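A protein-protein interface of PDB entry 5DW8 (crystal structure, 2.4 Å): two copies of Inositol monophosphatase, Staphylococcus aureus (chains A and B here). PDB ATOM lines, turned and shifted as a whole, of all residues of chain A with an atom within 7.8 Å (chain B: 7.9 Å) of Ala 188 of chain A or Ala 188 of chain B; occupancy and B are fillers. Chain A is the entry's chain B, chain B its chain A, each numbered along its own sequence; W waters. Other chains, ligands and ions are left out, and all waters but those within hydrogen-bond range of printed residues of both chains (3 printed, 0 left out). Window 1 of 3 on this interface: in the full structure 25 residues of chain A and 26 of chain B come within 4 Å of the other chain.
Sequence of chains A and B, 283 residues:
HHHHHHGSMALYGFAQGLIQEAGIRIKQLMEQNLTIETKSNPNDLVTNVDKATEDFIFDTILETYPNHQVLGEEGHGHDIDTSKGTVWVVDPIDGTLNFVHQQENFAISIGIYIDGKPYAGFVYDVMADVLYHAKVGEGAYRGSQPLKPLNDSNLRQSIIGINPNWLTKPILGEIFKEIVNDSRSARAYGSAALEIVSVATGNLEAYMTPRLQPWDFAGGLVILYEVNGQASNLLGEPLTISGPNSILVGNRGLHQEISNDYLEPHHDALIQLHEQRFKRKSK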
ATOM      1  N   ASN A  98      11.717  20.935  -4.158  1.00  0.00           N
ATOM      2  CA  ASN A  98      10.969  21.521  -5.247  1.00  0.00           C
ATOM      3  C   ASN A  98      11.510  20.996  -6.572  1.00  0.00           C
ATOM      4  O   ASN A  98      10.758  20.822  -7.504  1.00  0.00           O
ATOM      5  CB  ASN A  98      11.068  23.030  -5.229  1.00  0.00           C
ATOM      6  CG  ASN A  98      10.401  23.660  -4.027  1.00  0.00           C
ATOM      7  OD1 ASN A  98       9.681  23.014  -3.251  1.00  0.00           O
ATOM      8  ND2 ASN A  98      10.605  24.965  -3.889  1.00  0.00           N
ATOM      9  N   GLN A 102       8.547  19.480  -8.361  1.00  0.00           N
ATOM     10  CA  GLN A 102       8.057  20.578  -9.186  1.00  0.00           C
ATOM     11  C   GLN A 102       8.893  20.895 -10.420  1.00  0.00           C
ATOM     12  O   GLN A 102       8.432  21.634 -11.290  1.00  0.00           O
ATOM     13  CB  GLN A 102       7.956  21.866  -8.371  1.00  0.00           C
ATOM     14  CG  GLN A 102       7.136  21.740  -7.118  1.00  0.00           C
ATOM     15  CD  GLN A 102       6.874  23.072  -6.454  1.00  0.00           C
ATOM     16  OE1 GLN A 102       7.545  24.059  -6.734  1.00  0.00           O
ATOM     17  NE2 GLN A 102       5.892  23.097  -5.539  1.00  0.00           N
ATOM     18  N   ILE A 159       3.404  40.596   4.378  1.00  0.00           N
ATOM     19  CA  ILE A 159       3.302  39.169   4.114  1.00  0.00           C
ATOM     20  C   ILE A 159       4.615  38.577   4.552  1.00  0.00           C
ATOM     21  O   ILE A 159       5.663  39.105   4.249  1.00  0.00           O
ATOM     22  CB  ILE A 159       3.024  38.850   2.610  1.00  0.00           C
ATOM     23  CG1 ILE A 159       1.926  39.758   2.079  1.00  0.00           C
ATOM     24  CG2 ILE A 159       2.628  37.386   2.451  1.00  0.00           C
ATOM     25  CD1 ILE A 159       1.058  39.148   1.031  1.00  0.00           C
ATOM     26  N   ILE A 160       4.579  37.476   5.260  1.00  0.00           N
ATOM     27  CA  ILE A 160       5.817  36.898   5.746  1.00  0.00           C
ATOM     28  C   ILE A 160       6.016  35.467   5.276  1.00  0.00           C
ATOM     29  O   ILE A 160       5.057  34.774   5.002  1.00  0.00           O
ATOM     30  CB  ILE A 160       5.869  36.951   7.269  1.00  0.00           C
ATOM     31  CG1 ILE A 160       4.759  36.109   7.869  1.00  0.00           C
ATOM     32  CG2 ILE A 160       5.762  38.390   7.724  1.00  0.00           C
ATOM     33  CD1 ILE A 160       4.762  36.172   9.362  1.00  0.00           C
ATOM     34  N   GLY A 161       7.283  35.065   5.148  1.00  0.00           N
ATOM     35  CA  GLY A 161       7.667  33.720   4.756  1.00  0.00           C
ATOM     36  C   GLY A 161       7.865  32.932   6.044  1.00  0.00           C
ATOM     37  O   GLY A 161       8.779  33.230   6.823  1.00  0.00           O
ATOM     38  N   ILE A 162       6.991  31.962   6.293  1.00  0.00           N
ATOM     39  CA  ILE A 162       7.196  31.012   7.383  1.00  0.00           C
ATOM     40  C   ILE A 162       6.516  29.697   7.082  1.00  0.00           C
ATOM     41  O   ILE A 162       5.335  29.629   6.770  1.00  0.00           O
ATOM     42  CB  ILE A 162       6.739  31.554   8.771  1.00  0.00           C
ATOM     43  CG1 ILE A 162       7.237  30.657   9.905  1.00  0.00           C
ATOM     44  CG2 ILE A 162       5.242  31.673   8.866  1.00  0.00           C
ATOM     45  CD1 ILE A 162       6.996  31.270  11.275  1.00  0.00           C
ATOM     46  N   ASN A 163       7.285  28.637   7.191  1.00  0.00           N
ATOM     47  CA  ASN A 163       6.793  27.339   6.837  1.00  0.00           C
ATOM     48  C   ASN A 163       5.824  26.744   7.896  1.00  0.00           C
ATOM     49  O   ASN A 163       6.028  26.903   9.094  1.00  0.00           O
ATOM     50  CB  ASN A 163       7.961  26.401   6.574  1.00  0.00           C
ATOM     51  CG  ASN A 163       7.531  25.187   5.783  1.00  0.00           C
ATOM     52  OD1 ASN A 163       7.687  25.144   4.567  1.00  0.00           O
ATOM     53  ND2 ASN A 163       6.947  24.212   6.468  1.00  0.00           N
ATOM     54  N   PRO A 164       4.745  26.079   7.447  1.00  0.00           N
ATOM     55  CA  PRO A 164       3.800  25.524   8.420  1.00  0.00           C
ATOM     56  C   PRO A 164       4.447  24.670   9.511  1.00  0.00           C
ATOM     57  O   PRO A 164       4.015  24.714  10.683  1.00  0.00           O
ATOM     58  CB  PRO A 164       2.883  24.691   7.529  1.00  0.00           C
ATOM     59  CG  PRO A 164       2.790  25.520   6.321  1.00  0.00           C
ATOM     60  CD  PRO A 164       4.170  26.055   6.090  1.00  0.00           C
ATOM     61  N   ASN A 165       5.459  23.889   9.115  1.00  0.00           N
ATOM     62  CA  ASN A 165       6.195  23.040  10.033  1.00  0.00           C
ATOM     63  C   ASN A 165       6.565  23.803  11.336  1.00  0.00           C
ATOM     64  O   ASN A 165       6.467  23.258  12.421  1.00  0.00           O
ATOM     65  CB  ASN A 165       7.433  22.404   9.359  1.00  0.00           C
ATOM     66  CG  ASN A 165       7.079  21.306   8.305  1.00  0.00           C
ATOM     67  OD1 ASN A 165       6.792  20.153   8.656  1.00  0.00           O
ATOM     68  ND2 ASN A 165       7.151  21.652   6.994  1.00  0.00           N
ATOM     69  N   SER A 185      -0.769  38.157   5.877  1.00  0.00           N
ATOM     70  CA  SER A 185      -0.833  36.742   5.562  1.00  0.00           C
ATOM     71  C   SER A 185       0.598  36.148   5.519  1.00  0.00           C
ATOM     72  O   SER A 185       1.599  36.871   5.585  1.00  0.00           O
ATOM     73  CB  SER A 185      -1.572  36.442   4.220  1.00  0.00           C
ATOM     74  OG  SER A 185      -1.658  35.008   3.988  1.00  0.00           O
ATOM     75  N   ALA A 186       0.657  34.820   5.429  1.00  0.00           N
ATOM     76  CA  ALA A 186       1.918  34.115   5.340  1.00  0.00           C
ATOM     77  C   ALA A 186       1.977  33.232   4.071  1.00  0.00           C
ATOM     78  O   ALA A 186       0.962  32.929   3.438  1.00  0.00           O
ATOM     79  CB  ALA A 186       2.158  33.295   6.598  1.00  0.00           C
ATOM     80  N   ARG A 187       3.199  32.890   3.712  1.00  0.00           N
ATOM     81  CA  ARG A 187       3.531  32.094   2.567  1.00  0.00           C
ATOM     82  C   ARG A 187       4.711  31.196   2.989  1.00  0.00           C
ATOM     83  O   ARG A 187       5.458  31.526   3.934  1.00  0.00           O
ATOM     84  CB  ARG A 187       4.028  32.993   1.400  1.00  0.00           C
ATOM     85  CG  ARG A 187       3.088  34.068   0.877  1.00  0.00           C
ATOM     86  CD  ARG A 187       1.856  33.483   0.204  1.00  0.00           C
ATOM     87  NE  ARG A 187       0.895  34.504  -0.227  1.00  0.00           N
ATOM     88  CZ  ARG A 187      -0.172  34.897   0.478  1.00  0.00           C
ATOM     89  NH1 ARG A 187      -0.479  34.366   1.692  1.00  0.00           N
ATOM     90  NH2 ARG A 187      -0.958  35.835  -0.053  1.00  0.00           N
ATOM     91  N   ALA A 188       4.889  30.095   2.259  1.00  0.00           N
ATOM     92  CA  ALA A 188       6.051  29.229   2.375  1.00  0.00           C
ATOM     93  C   ALA A 188       6.418  28.739   0.972  1.00  0.00           C
ATOM     94  O   ALA A 188       5.554  28.188   0.280  1.00  0.00           O
ATOM     95  CB  ALA A 188       5.726  28.063   3.268  1.00  0.00           C
ATOM     96  N   TYR A 189       7.656  28.927   0.530  1.00  0.00           N
ATOM     97  CA  TYR A 189       8.048  28.478  -0.824  1.00  0.00           C
ATOM     98  C   TYR A 189       9.017  27.295  -0.937  1.00  0.00           C
ATOM     99  O   TYR A 189       9.228  26.806  -2.021  1.00  0.00           O
ATOM    100  CB  TYR A 189       8.668  29.632  -1.625  1.00  0.00           C
ATOM    101  CG  TYR A 189       7.813  30.847  -1.754  1.00  0.00           C
ATOM    102  CD1 TYR A 189       6.456  30.713  -1.917  1.00  0.00           C
ATOM    103  CD2 TYR A 189       8.367  32.147  -1.764  1.00  0.00           C
ATOM    104  CE1 TYR A 189       5.651  31.804  -2.089  1.00  0.00           C
ATOM    105  CE2 TYR A 189       7.540  33.261  -1.952  1.00  0.00           C
ATOM    106  CZ  TYR A 189       6.168  33.060  -2.097  1.00  0.00           C
ATOM    107  OH  TYR A 189       5.226  34.060  -2.230  1.00  0.00           O
ATOM    108  N   GLY A 190       9.644  26.858   0.140  1.00  0.00           N
ATOM    109  CA  GLY A 190      10.526  25.679   0.024  1.00  0.00           C
ATOM    110  C   GLY A 190      11.953  25.952  -0.444  1.00  0.00           C
ATOM    111  O   GLY A 190      12.741  25.025  -0.592  1.00  0.00           O
ATOM    112  N   SER A 191      12.283  27.224  -0.674  1.00  0.00           N
ATOM    113  CA  SER A 191      13.663  27.636  -0.872  1.00  0.00           C
ATOM    114  C   SER A 191      13.992  28.795   0.013  1.00  0.00           C
ATOM    115  O   SER A 191      13.366  29.838  -0.090  1.00  0.00           O
ATOM    116  CB  SER A 191      13.921  28.087  -2.314  1.00  0.00           C
ATOM    117  OG  SER A 191      15.233  28.594  -2.408  1.00  0.00           O
ATOM    118  N   GLU A 195      13.502  32.794  -0.982  1.00  0.00           N
ATOM    119  CA  GLU A 195      12.725  33.536   0.023  1.00  0.00           C
ATOM    120  C   GLU A 195      13.447  34.702   0.668  1.00  0.00           C
ATOM    121  O   GLU A 195      12.817  35.721   0.989  1.00  0.00           O
ATOM    122  CB  GLU A 195      12.217  32.604   1.088  1.00  0.00           C
ATOM    123  CG  GLU A 195      11.059  31.835   0.537  1.00  0.00           C
ATOM    124  CD  GLU A 195      10.610  30.772   1.460  1.00  0.00           C
ATOM    125  OE1 GLU A 195      11.283  29.755   1.566  1.00  0.00           O
ATOM    126  OE2 GLU A 195       9.576  30.977   2.065  1.00  0.00           O
ATOM    127  N   LEU A 204       8.263  39.528  -0.403  1.00  0.00           N
ATOM    128  CA  LEU A 204       7.853  39.251   0.995  1.00  0.00           C
ATOM    129  C   LEU A 204       8.447  40.396   1.788  1.00  0.00           C
ATOM    130  O   LEU A 204       9.494  40.879   1.436  1.00  0.00           O
ATOM    131  CB  LEU A 204       8.423  37.926   1.573  1.00  0.00           C
ATOM    132  CG  LEU A 204       8.015  36.588   0.917  1.00  0.00           C
ATOM    133  CD1 LEU A 204       8.917  35.426   1.307  1.00  0.00           C
ATOM    134  CD2 LEU A 204       6.559  36.249   1.177  1.00  0.00           C
ATOM    135  N   TYR A 207      10.990  37.106   6.291  1.00  0.00           N
ATOM    136  CA  TYR A 207      11.095  35.670   6.247  1.00  0.00           C
ATOM    137  C   TYR A 207      11.865  35.148   7.486  1.00  0.00           C
ATOM    138  O   TYR A 207      12.905  35.703   7.887  1.00  0.00           O
ATOM    139  CB  TYR A 207      11.775  35.256   4.946  1.00  0.00           C
ATOM    140  CG  TYR A 207      12.360  33.868   4.920  1.00  0.00           C
ATOM    141  CD1 TYR A 207      11.540  32.727   4.889  1.00  0.00           C
ATOM    142  CD2 TYR A 207      13.722  33.684   4.902  1.00  0.00           C
ATOM    143  CE1 TYR A 207      12.079  31.447   4.835  1.00  0.00           C
ATOM    144  CE2 TYR A 207      14.280  32.413   4.852  1.00  0.00           C
ATOM    145  CZ  TYR A 207      13.453  31.306   4.805  1.00  0.00           C
ATOM    146  OH  TYR A 207      14.033  30.064   4.769  1.00  0.00           O
ATOM    147  N   ASN B  98      -1.589  38.914  -2.847  1.00  0.00           N
ATOM    148  CA  ASN B  98      -0.431  38.717  -3.714  1.00  0.00           C
ATOM    149  C   ASN B  98      -0.444  39.796  -4.779  1.00  0.00           C
ATOM    150  O   ASN B  98       0.583  40.391  -5.089  1.00  0.00           O
ATOM    151  CB  ASN B  98      -0.464  37.347  -4.423  1.00  0.00           C
ATOM    152  CG  ASN B  98      -0.206  36.154  -3.494  1.00  0.00           C
ATOM    153  OD1 ASN B  98       0.211  36.276  -2.337  1.00  0.00           O
ATOM    154  ND2 ASN B  98      -0.463  34.972  -4.023  1.00  0.00           N
ATOM    155  N   GLN B 102       2.804  41.645  -4.226  1.00  0.00           N
ATOM    156  CA  GLN B 102       3.730  40.986  -5.135  1.00  0.00           C
ATOM    157  C   GLN B 102       3.530  41.412  -6.608  1.00  0.00           C
ATOM    158  O   GLN B 102       4.437  41.273  -7.414  1.00  0.00           O
ATOM    159  CB  GLN B 102       3.556  39.462  -5.020  1.00  0.00           C
ATOM    160  CG  GLN B 102       3.465  38.933  -3.592  1.00  0.00           C
ATOM    161  CD  GLN B 102       3.655  37.418  -3.522  1.00  0.00           C
ATOM    162  OE1 GLN B 102       3.084  36.685  -4.328  1.00  0.00           O
ATOM    163  NE2 GLN B 102       4.463  36.945  -2.574  1.00  0.00           N
ATOM    164  N   ILE B 159       4.274  16.836  -0.908  1.00  0.00           N
ATOM    165  CA  ILE B 159       4.324  18.260  -0.544  1.00  0.00           C
ATOM    166  C   ILE B 159       2.888  18.818  -0.582  1.00  0.00           C
ATOM    167  O   ILE B 159       2.162  18.625  -1.552  1.00  0.00           O
ATOM    168  CB  ILE B 159       5.241  19.018  -1.480  1.00  0.00           C
ATOM    169  CG1 ILE B 159       6.677  18.751  -1.082  1.00  0.00           C
ATOM    170  CG2 ILE B 159       5.026  20.510  -1.378  1.00  0.00           C
ATOM    171  CD1 ILE B 159       7.612  18.868  -2.241  1.00  0.00           C
ATOM    172  N   ILE B 160       2.492  19.487   0.496  1.00  0.00           N
ATOM    173  CA  ILE B 160       1.106  19.788   0.708  1.00  0.00           C
ATOM    174  C   ILE B 160       0.991  21.267   0.704  1.00  0.00           C
ATOM    175  O   ILE B 160       1.900  21.945   1.144  1.00  0.00           O
ATOM    176  CB  ILE B 160       0.548  19.202   2.046  1.00  0.00           C
ATOM    177  CG1 ILE B 160       1.339  19.669   3.264  1.00  0.00           C
ATOM    178  CG2 ILE B 160       0.559  17.699   2.005  1.00  0.00           C
ATOM    179  CD1 ILE B 160       0.646  19.376   4.591  1.00  0.00           C
ATOM    180  N   GLY B 161      -0.128  21.760   0.204  1.00  0.00           N
ATOM    181  CA  GLY B 161      -0.390  23.180   0.166  1.00  0.00           C
ATOM    182  C   GLY B 161      -1.283  23.486   1.343  1.00  0.00           C
ATOM    183  O   GLY B 161      -2.448  23.086   1.358  1.00  0.00           O
ATOM    184  N   ILE B 162      -0.744  24.169   2.342  1.00  0.00           N
ATOM    185  CA  ILE B 162      -1.545  24.598   3.456  1.00  0.00           C
ATOM    186  C   ILE B 162      -0.964  25.848   4.097  1.00  0.00           C
ATOM    187  O   ILE B 162       0.262  25.953   4.303  1.00  0.00           O
ATOM    188  CB  ILE B 162      -1.701  23.472   4.487  1.00  0.00           C
ATOM    189  CG1 ILE B 162      -2.822  23.808   5.480  1.00  0.00           C
ATOM    190  CG2 ILE B 162      -0.421  23.288   5.254  1.00  0.00           C
ATOM    191  CD1 ILE B 162      -3.251  22.642   6.359  1.00  0.00           C
ATOM    192  N   ASN B 163      -1.849  26.806   4.399  1.00  0.00           N
ATOM    193  CA  ASN B 163      -1.435  28.089   5.004  1.00  0.00           C
ATOM    194  C   ASN B 163      -1.106  28.034   6.496  1.00  0.00           C
ATOM    195  O   ASN B 163      -1.905  27.560   7.269  1.00  0.00           O
ATOM    196  CB  ASN B 163      -2.489  29.169   4.777  1.00  0.00           C
ATOM    197  CG  ASN B 163      -1.907  30.579   4.845  1.00  0.00           C
ATOM    198  OD1 ASN B 163      -1.586  31.177   3.854  1.00  0.00           O
ATOM    199  ND2 ASN B 163      -1.814  31.108   6.026  1.00  0.00           N
ATOM    200  N   PRO B 164       0.048  28.609   6.902  1.00  0.00           N
ATOM    201  CA  PRO B 164       0.364  28.656   8.329  1.00  0.00           C
ATOM    202  C   PRO B 164      -0.764  29.195   9.210  1.00  0.00           C
ATOM    203  O   PRO B 164      -0.952  28.700  10.311  1.00  0.00           O
ATOM    204  CB  PRO B 164       1.601  29.548   8.394  1.00  0.00           C
ATOM    205  CG  PRO B 164       2.225  29.443   7.066  1.00  0.00           C
ATOM    206  CD  PRO B 164       1.117  29.215   6.086  1.00  0.00           C
ATOM    207  N   ASN B 165      -1.537  30.169   8.740  1.00  0.00           N
ATOM    208  CA  ASN B 165      -2.622  30.716   9.573  1.00  0.00           C
ATOM    209  C   ASN B 165      -3.579  29.626  10.077  1.00  0.00           C
ATOM    210  O   ASN B 165      -4.186  29.795  11.108  1.00  0.00           O
ATOM    211  CB  ASN B 165      -3.448  31.801   8.853  1.00  0.00           C
ATOM    212  CG  ASN B 165      -2.708  33.147   8.712  1.00  0.00           C
ATOM    213  OD1 ASN B 165      -2.990  34.106   9.459  1.00  0.00           O
ATOM    214  ND2 ASN B 165      -1.797  33.249   7.732  1.00  0.00           N
ATOM    215  N   SER B 185       6.700  17.923   3.181  1.00  0.00           N
ATOM    216  CA  SER B 185       6.869  19.365   3.424  1.00  0.00           C
ATOM    217  C   SER B 185       5.641  20.190   3.000  1.00  0.00           C
ATOM    218  O   SER B 185       4.778  19.722   2.255  1.00  0.00           O
ATOM    219  CB  SER B 185       8.112  19.908   2.707  1.00  0.00           C
ATOM    220  OG  SER B 185       8.417  21.229   3.150  1.00  0.00           O
ATOM    221  N   ALA B 186       5.602  21.429   3.476  1.00  0.00           N
ATOM    222  CA  ALA B 186       4.466  22.320   3.295  1.00  0.00           C
ATOM    223  C   ALA B 186       4.834  23.604   2.570  1.00  0.00           C
ATOM    224  O   ALA B 186       5.971  24.077   2.656  1.00  0.00           O
ATOM    225  CB  ALA B 186       3.841  22.628   4.621  1.00  0.00           C
ATOM    226  N   ARG B 187       3.853  24.113   1.831  1.00  0.00           N
ATOM    227  CA  ARG B 187       3.925  25.310   1.009  1.00  0.00           C
ATOM    228  C   ARG B 187       2.637  26.124   1.214  1.00  0.00           C
ATOM    229  O   ARG B 187       1.589  25.610   1.639  1.00  0.00           O
ATOM    230  CB  ARG B 187       3.975  24.955  -0.488  1.00  0.00           C
ATOM    231  CG  ARG B 187       5.105  24.047  -0.930  1.00  0.00           C
ATOM    232  CD  ARG B 187       6.428  24.763  -0.793  1.00  0.00           C
ATOM    233  NE  ARG B 187       7.605  23.967  -1.166  1.00  0.00           N
ATOM    234  CZ  ARG B 187       8.285  23.171  -0.350  1.00  0.00           C
ATOM    235  NH1 ARG B 187       7.891  22.976   0.900  1.00  0.00           N
ATOM    236  NH2 ARG B 187       9.351  22.535  -0.803  1.00  0.00           N
ATOM    237  N   ALA B 188       2.714  27.387   0.833  1.00  0.00           N
ATOM    238  CA  ALA B 188       1.587  28.277   0.884  1.00  0.00           C
ATOM    239  C   ALA B 188       1.771  29.374  -0.177  1.00  0.00           C
ATOM    240  O   ALA B 188       2.622  30.234  -0.036  1.00  0.00           O
ATOM    241  CB  ALA B 188       1.539  28.865   2.259  1.00  0.00           C
ATOM    242  N   TYR B 189       1.015  29.321  -1.264  1.00  0.00           N
ATOM    243  CA  TYR B 189       1.215  30.290  -2.350  1.00  0.00           C
ATOM    244  C   TYR B 189       0.236  31.471  -2.344  1.00  0.00           C
ATOM    245  O   TYR B 189       0.498  32.479  -2.993  1.00  0.00           O
ATOM    246  CB  TYR B 189       1.230  29.589  -3.720  1.00  0.00           C
ATOM    247  CG  TYR B 189       2.317  28.579  -3.837  1.00  0.00           C
ATOM    248  CD1 TYR B 189       3.641  28.935  -3.641  1.00  0.00           C
ATOM    249  CD2 TYR B 189       2.045  27.259  -4.179  1.00  0.00           C
ATOM    250  CE1 TYR B 189       4.655  28.013  -3.778  1.00  0.00           C
ATOM    251  CE2 TYR B 189       3.060  26.318  -4.316  1.00  0.00           C
ATOM    252  CZ  TYR B 189       4.360  26.697  -4.093  1.00  0.00           C
ATOM    253  OH  TYR B 189       5.390  25.779  -4.230  1.00  0.00           O
ATOM    254  N   GLY B 190      -0.880  31.352  -1.630  1.00  0.00           N
ATOM    255  CA  GLY B 190      -1.808  32.474  -1.446  1.00  0.00           C
ATOM    256  C   GLY B 190      -2.836  32.663  -2.553  1.00  0.00           C
ATOM    257  O   GLY B 190      -3.437  33.714  -2.654  1.00  0.00           O
ATOM    258  N   SER B 191      -3.029  31.643  -3.379  1.00  0.00           N
ATOM    259  CA  SER B 191      -4.073  31.621  -4.393  1.00  0.00           C
ATOM    260  C   SER B 191      -4.591  30.210  -4.498  1.00  0.00           C
ATOM    261  O   SER B 191      -3.857  29.321  -4.914  1.00  0.00           O
ATOM    262  CB  SER B 191      -3.514  32.046  -5.739  1.00  0.00           C
ATOM    263  OG  SER B 191      -4.465  31.887  -6.775  1.00  0.00           O
ATOM    264  N   GLU B 195      -3.270  26.972  -6.679  1.00  0.00           N
ATOM    265  CA  GLU B 195      -2.863  25.815  -5.878  1.00  0.00           C
ATOM    266  C   GLU B 195      -3.617  24.523  -6.269  1.00  0.00           C
ATOM    267  O   GLU B 195      -3.013  23.449  -6.322  1.00  0.00           O
ATOM    268  CB  GLU B 195      -2.940  26.137  -4.367  1.00  0.00           C
ATOM    269  CG  GLU B 195      -1.743  26.942  -3.868  1.00  0.00           C
ATOM    270  CD  GLU B 195      -1.875  27.487  -2.441  1.00  0.00           C
ATOM    271  OE1 GLU B 195      -2.474  28.559  -2.199  1.00  0.00           O
ATOM    272  OE2 GLU B 195      -1.336  26.853  -1.529  1.00  0.00           O
ATOM    273  N   LEU B 204       2.048  20.050  -6.515  1.00  0.00           N
ATOM    274  CA  LEU B 204       1.665  19.841  -5.120  1.00  0.00           C
ATOM    275  C   LEU B 204       0.876  18.533  -5.102  1.00  0.00           C
ATOM    276  O   LEU B 204       0.048  18.313  -5.963  1.00  0.00           O
ATOM    277  CB  LEU B 204       0.770  20.984  -4.591  1.00  0.00           C
ATOM    278  CG  LEU B 204       1.287  22.398  -4.257  1.00  0.00           C
ATOM    279  CD1 LEU B 204       0.116  23.213  -3.688  1.00  0.00           C
ATOM    280  CD2 LEU B 204       2.420  22.387  -3.253  1.00  0.00           C
ATOM    281  N   TYR B 207      -3.746  19.972  -1.562  1.00  0.00           N
ATOM    282  CA  TYR B 207      -4.026  21.334  -1.078  1.00  0.00           C
ATOM    283  C   TYR B 207      -5.281  21.318  -0.174  1.00  0.00           C
ATOM    284  O   TYR B 207      -6.239  20.554  -0.403  1.00  0.00           O
ATOM    285  CB  TYR B 207      -4.118  22.347  -2.234  1.00  0.00           C
ATOM    286  CG  TYR B 207      -4.757  23.669  -1.878  1.00  0.00           C
ATOM    287  CD1 TYR B 207      -4.125  24.571  -1.032  1.00  0.00           C
ATOM    288  CD2 TYR B 207      -6.014  24.018  -2.392  1.00  0.00           C
ATOM    289  CE1 TYR B 207      -4.731  25.787  -0.703  1.00  0.00           C
ATOM    290  CE2 TYR B 207      -6.603  25.220  -2.091  1.00  0.00           C
ATOM    291  CZ  TYR B 207      -5.975  26.116  -1.253  1.00  0.00           C
ATOM    292  OH  TYR B 207      -6.611  27.323  -0.947  1.00  0.00           O
HETATM  293  O   HOH W   1       7.703  26.655  -4.142  1.00  0.00           O
HETATM  294  O   HOH W   2      -3.096  36.277  -1.792  1.00  0.00           O
HETATM  295  O   HOH W   3      12.158  22.448  -1.637  1.00  0.00           O
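The backbone carbonyl oxygen of Tyr 189 of chain B is in hydrogen-bond range of the guanidinium group of Arg 187 of chain A (3.5 Å).
NE2 of Gln 102 of chain B sits at hydrogen-bond distance from OH of Tyr 189 of chain A (3.0 Å).
OH of Tyr 189 of chain B sits at hydrogen-bond distance from NE2 of Gln 102 of chain A (3.0 Å).
OD1 of Asn 163 of chain B sits close to O of Ala 186 of chain A, at 3.1 Å.
The backbone carbonyl oxygen of Ala 186 of chain B lies close to the side-chain amide oxygen of Asn 163 of chain A (2.8 Å).
The guanidinium group of Arg 187 of chain A is in hydrogen-bond range of the side-chain amide oxygen of Asn 98 of chain B (2.6 Å).
The side-chain amide oxygen (OD1) of Asn 98 of chain A lies within hydrogen-bond range of the guanidinium group (NH2) of Arg 187 of chain B.
N of Ala 188 of chain B lies within hydrogen-bond range of O of Ala 188 of chain A (3.0 Å).
O of Tyr 189 of chain A lies within hydrogen-bond range of NE of Arg 187 of chain B, at 3.4 Å.
Among the printed residues, pairs that only touch across the chains: Ile 162 of chain A with Pro 164 of chain B (3.1 Å), Pro 164 of chain A with Ile 162 of chain B (3.3 Å), Pro 164 of chain A with Ala 186 of chain B (3.5 Å), Asn 165 of chain A with Ala 186 of chain B (3.9 Å), Ser 185 of chain A with Asn 163 of chain B (3.8 Å), Ala 186 of chain A with Pro 164 of chain B (3.9 Å), Ala 186 of chain A with Asn 165 of chain B (3.7 Å), Arg 187 of chain A with Ala 188 of chain B (3.3 Å), Arg 187 of chain A with Gly 190 of chain B (3.5 Å), Ala 188 of chain A with Arg 187 of chain B (3.4 Å), Tyr 189 of chain A with Ala 188 of chain B (3.98 Å), Tyr 189 of chain A with Tyr 189 of chain B (3.7 Å) and Gly 190 of chain A with Arg 187 of chain B (3.4 Å).
The side-chain amide nitrogen of Asn 165 of chain B sits close to the side-chain amide nitrogen of Asn 163 of chain B (2.7 Å).
N of Tyr 189 of chain A is in hydrogen-bond range of OE2 of Glu 195 of chain A (3.2 Å).
Asn 163 of chain A touches Ala 186 of chain B, and with the chains exchanged Ala 186 of chain A touches Asn 163 of chain B.
19 positions are printed for both chains.
Of the 22 pairs that touch across the chains among the printed residues, 20 have their exchanged pair printed and touching as well.
Hydrophobic or aromatic side chains of chain B that line the printed part of chain A: Pro 164, Ala 186, Ala 188 and Tyr 189.
Printed residues of chain A that touch a printed residue of chain B: Asn 98, Gln 102, Ile 162, Asn 163, Pro 164, Asn 165, Ser 185, Ala 186, Arg 187, Ala 188, Tyr 189 and Gly 190.
Hydrophobic or aromatic side chains of chain A within 4 Å of the printed part of chain B: Pro 164, Ala 186, Ala 188 and Tyr 189.
Among the printed residues, 22 pairs touch across the chains.
Water W3 lies within hydrogen-bond range of the backbone carbonyl oxygen of Gly 190 of chain A (2.8 Å), the guanidinium group of Arg 187 of chain B (2.9 Å) and the backbone NH of Asn 98 of chain A (3.0 Å).
Ala 188 of chain A touches just these residues of chain B: Arg 187 and Ala 188.
Printed residues of chain A within 4 Å of Asn 165 of chain B: Ala 186 (3.7 Å).
Of the printed residues of chain B, Ile 162 of chain A touches Pro 164 (3.1 Å).
Ile 159 of chain A touches none of the printed residues of chain B.
The nearest printed residue of chain A that does not touch Ala 188 of chain B is Ala 186 of chain A (4.3 Å).
The nearest printed residue of chain A that does not touch Gly 190 of chain B is Ala 186 of chain A (5.6 Å).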
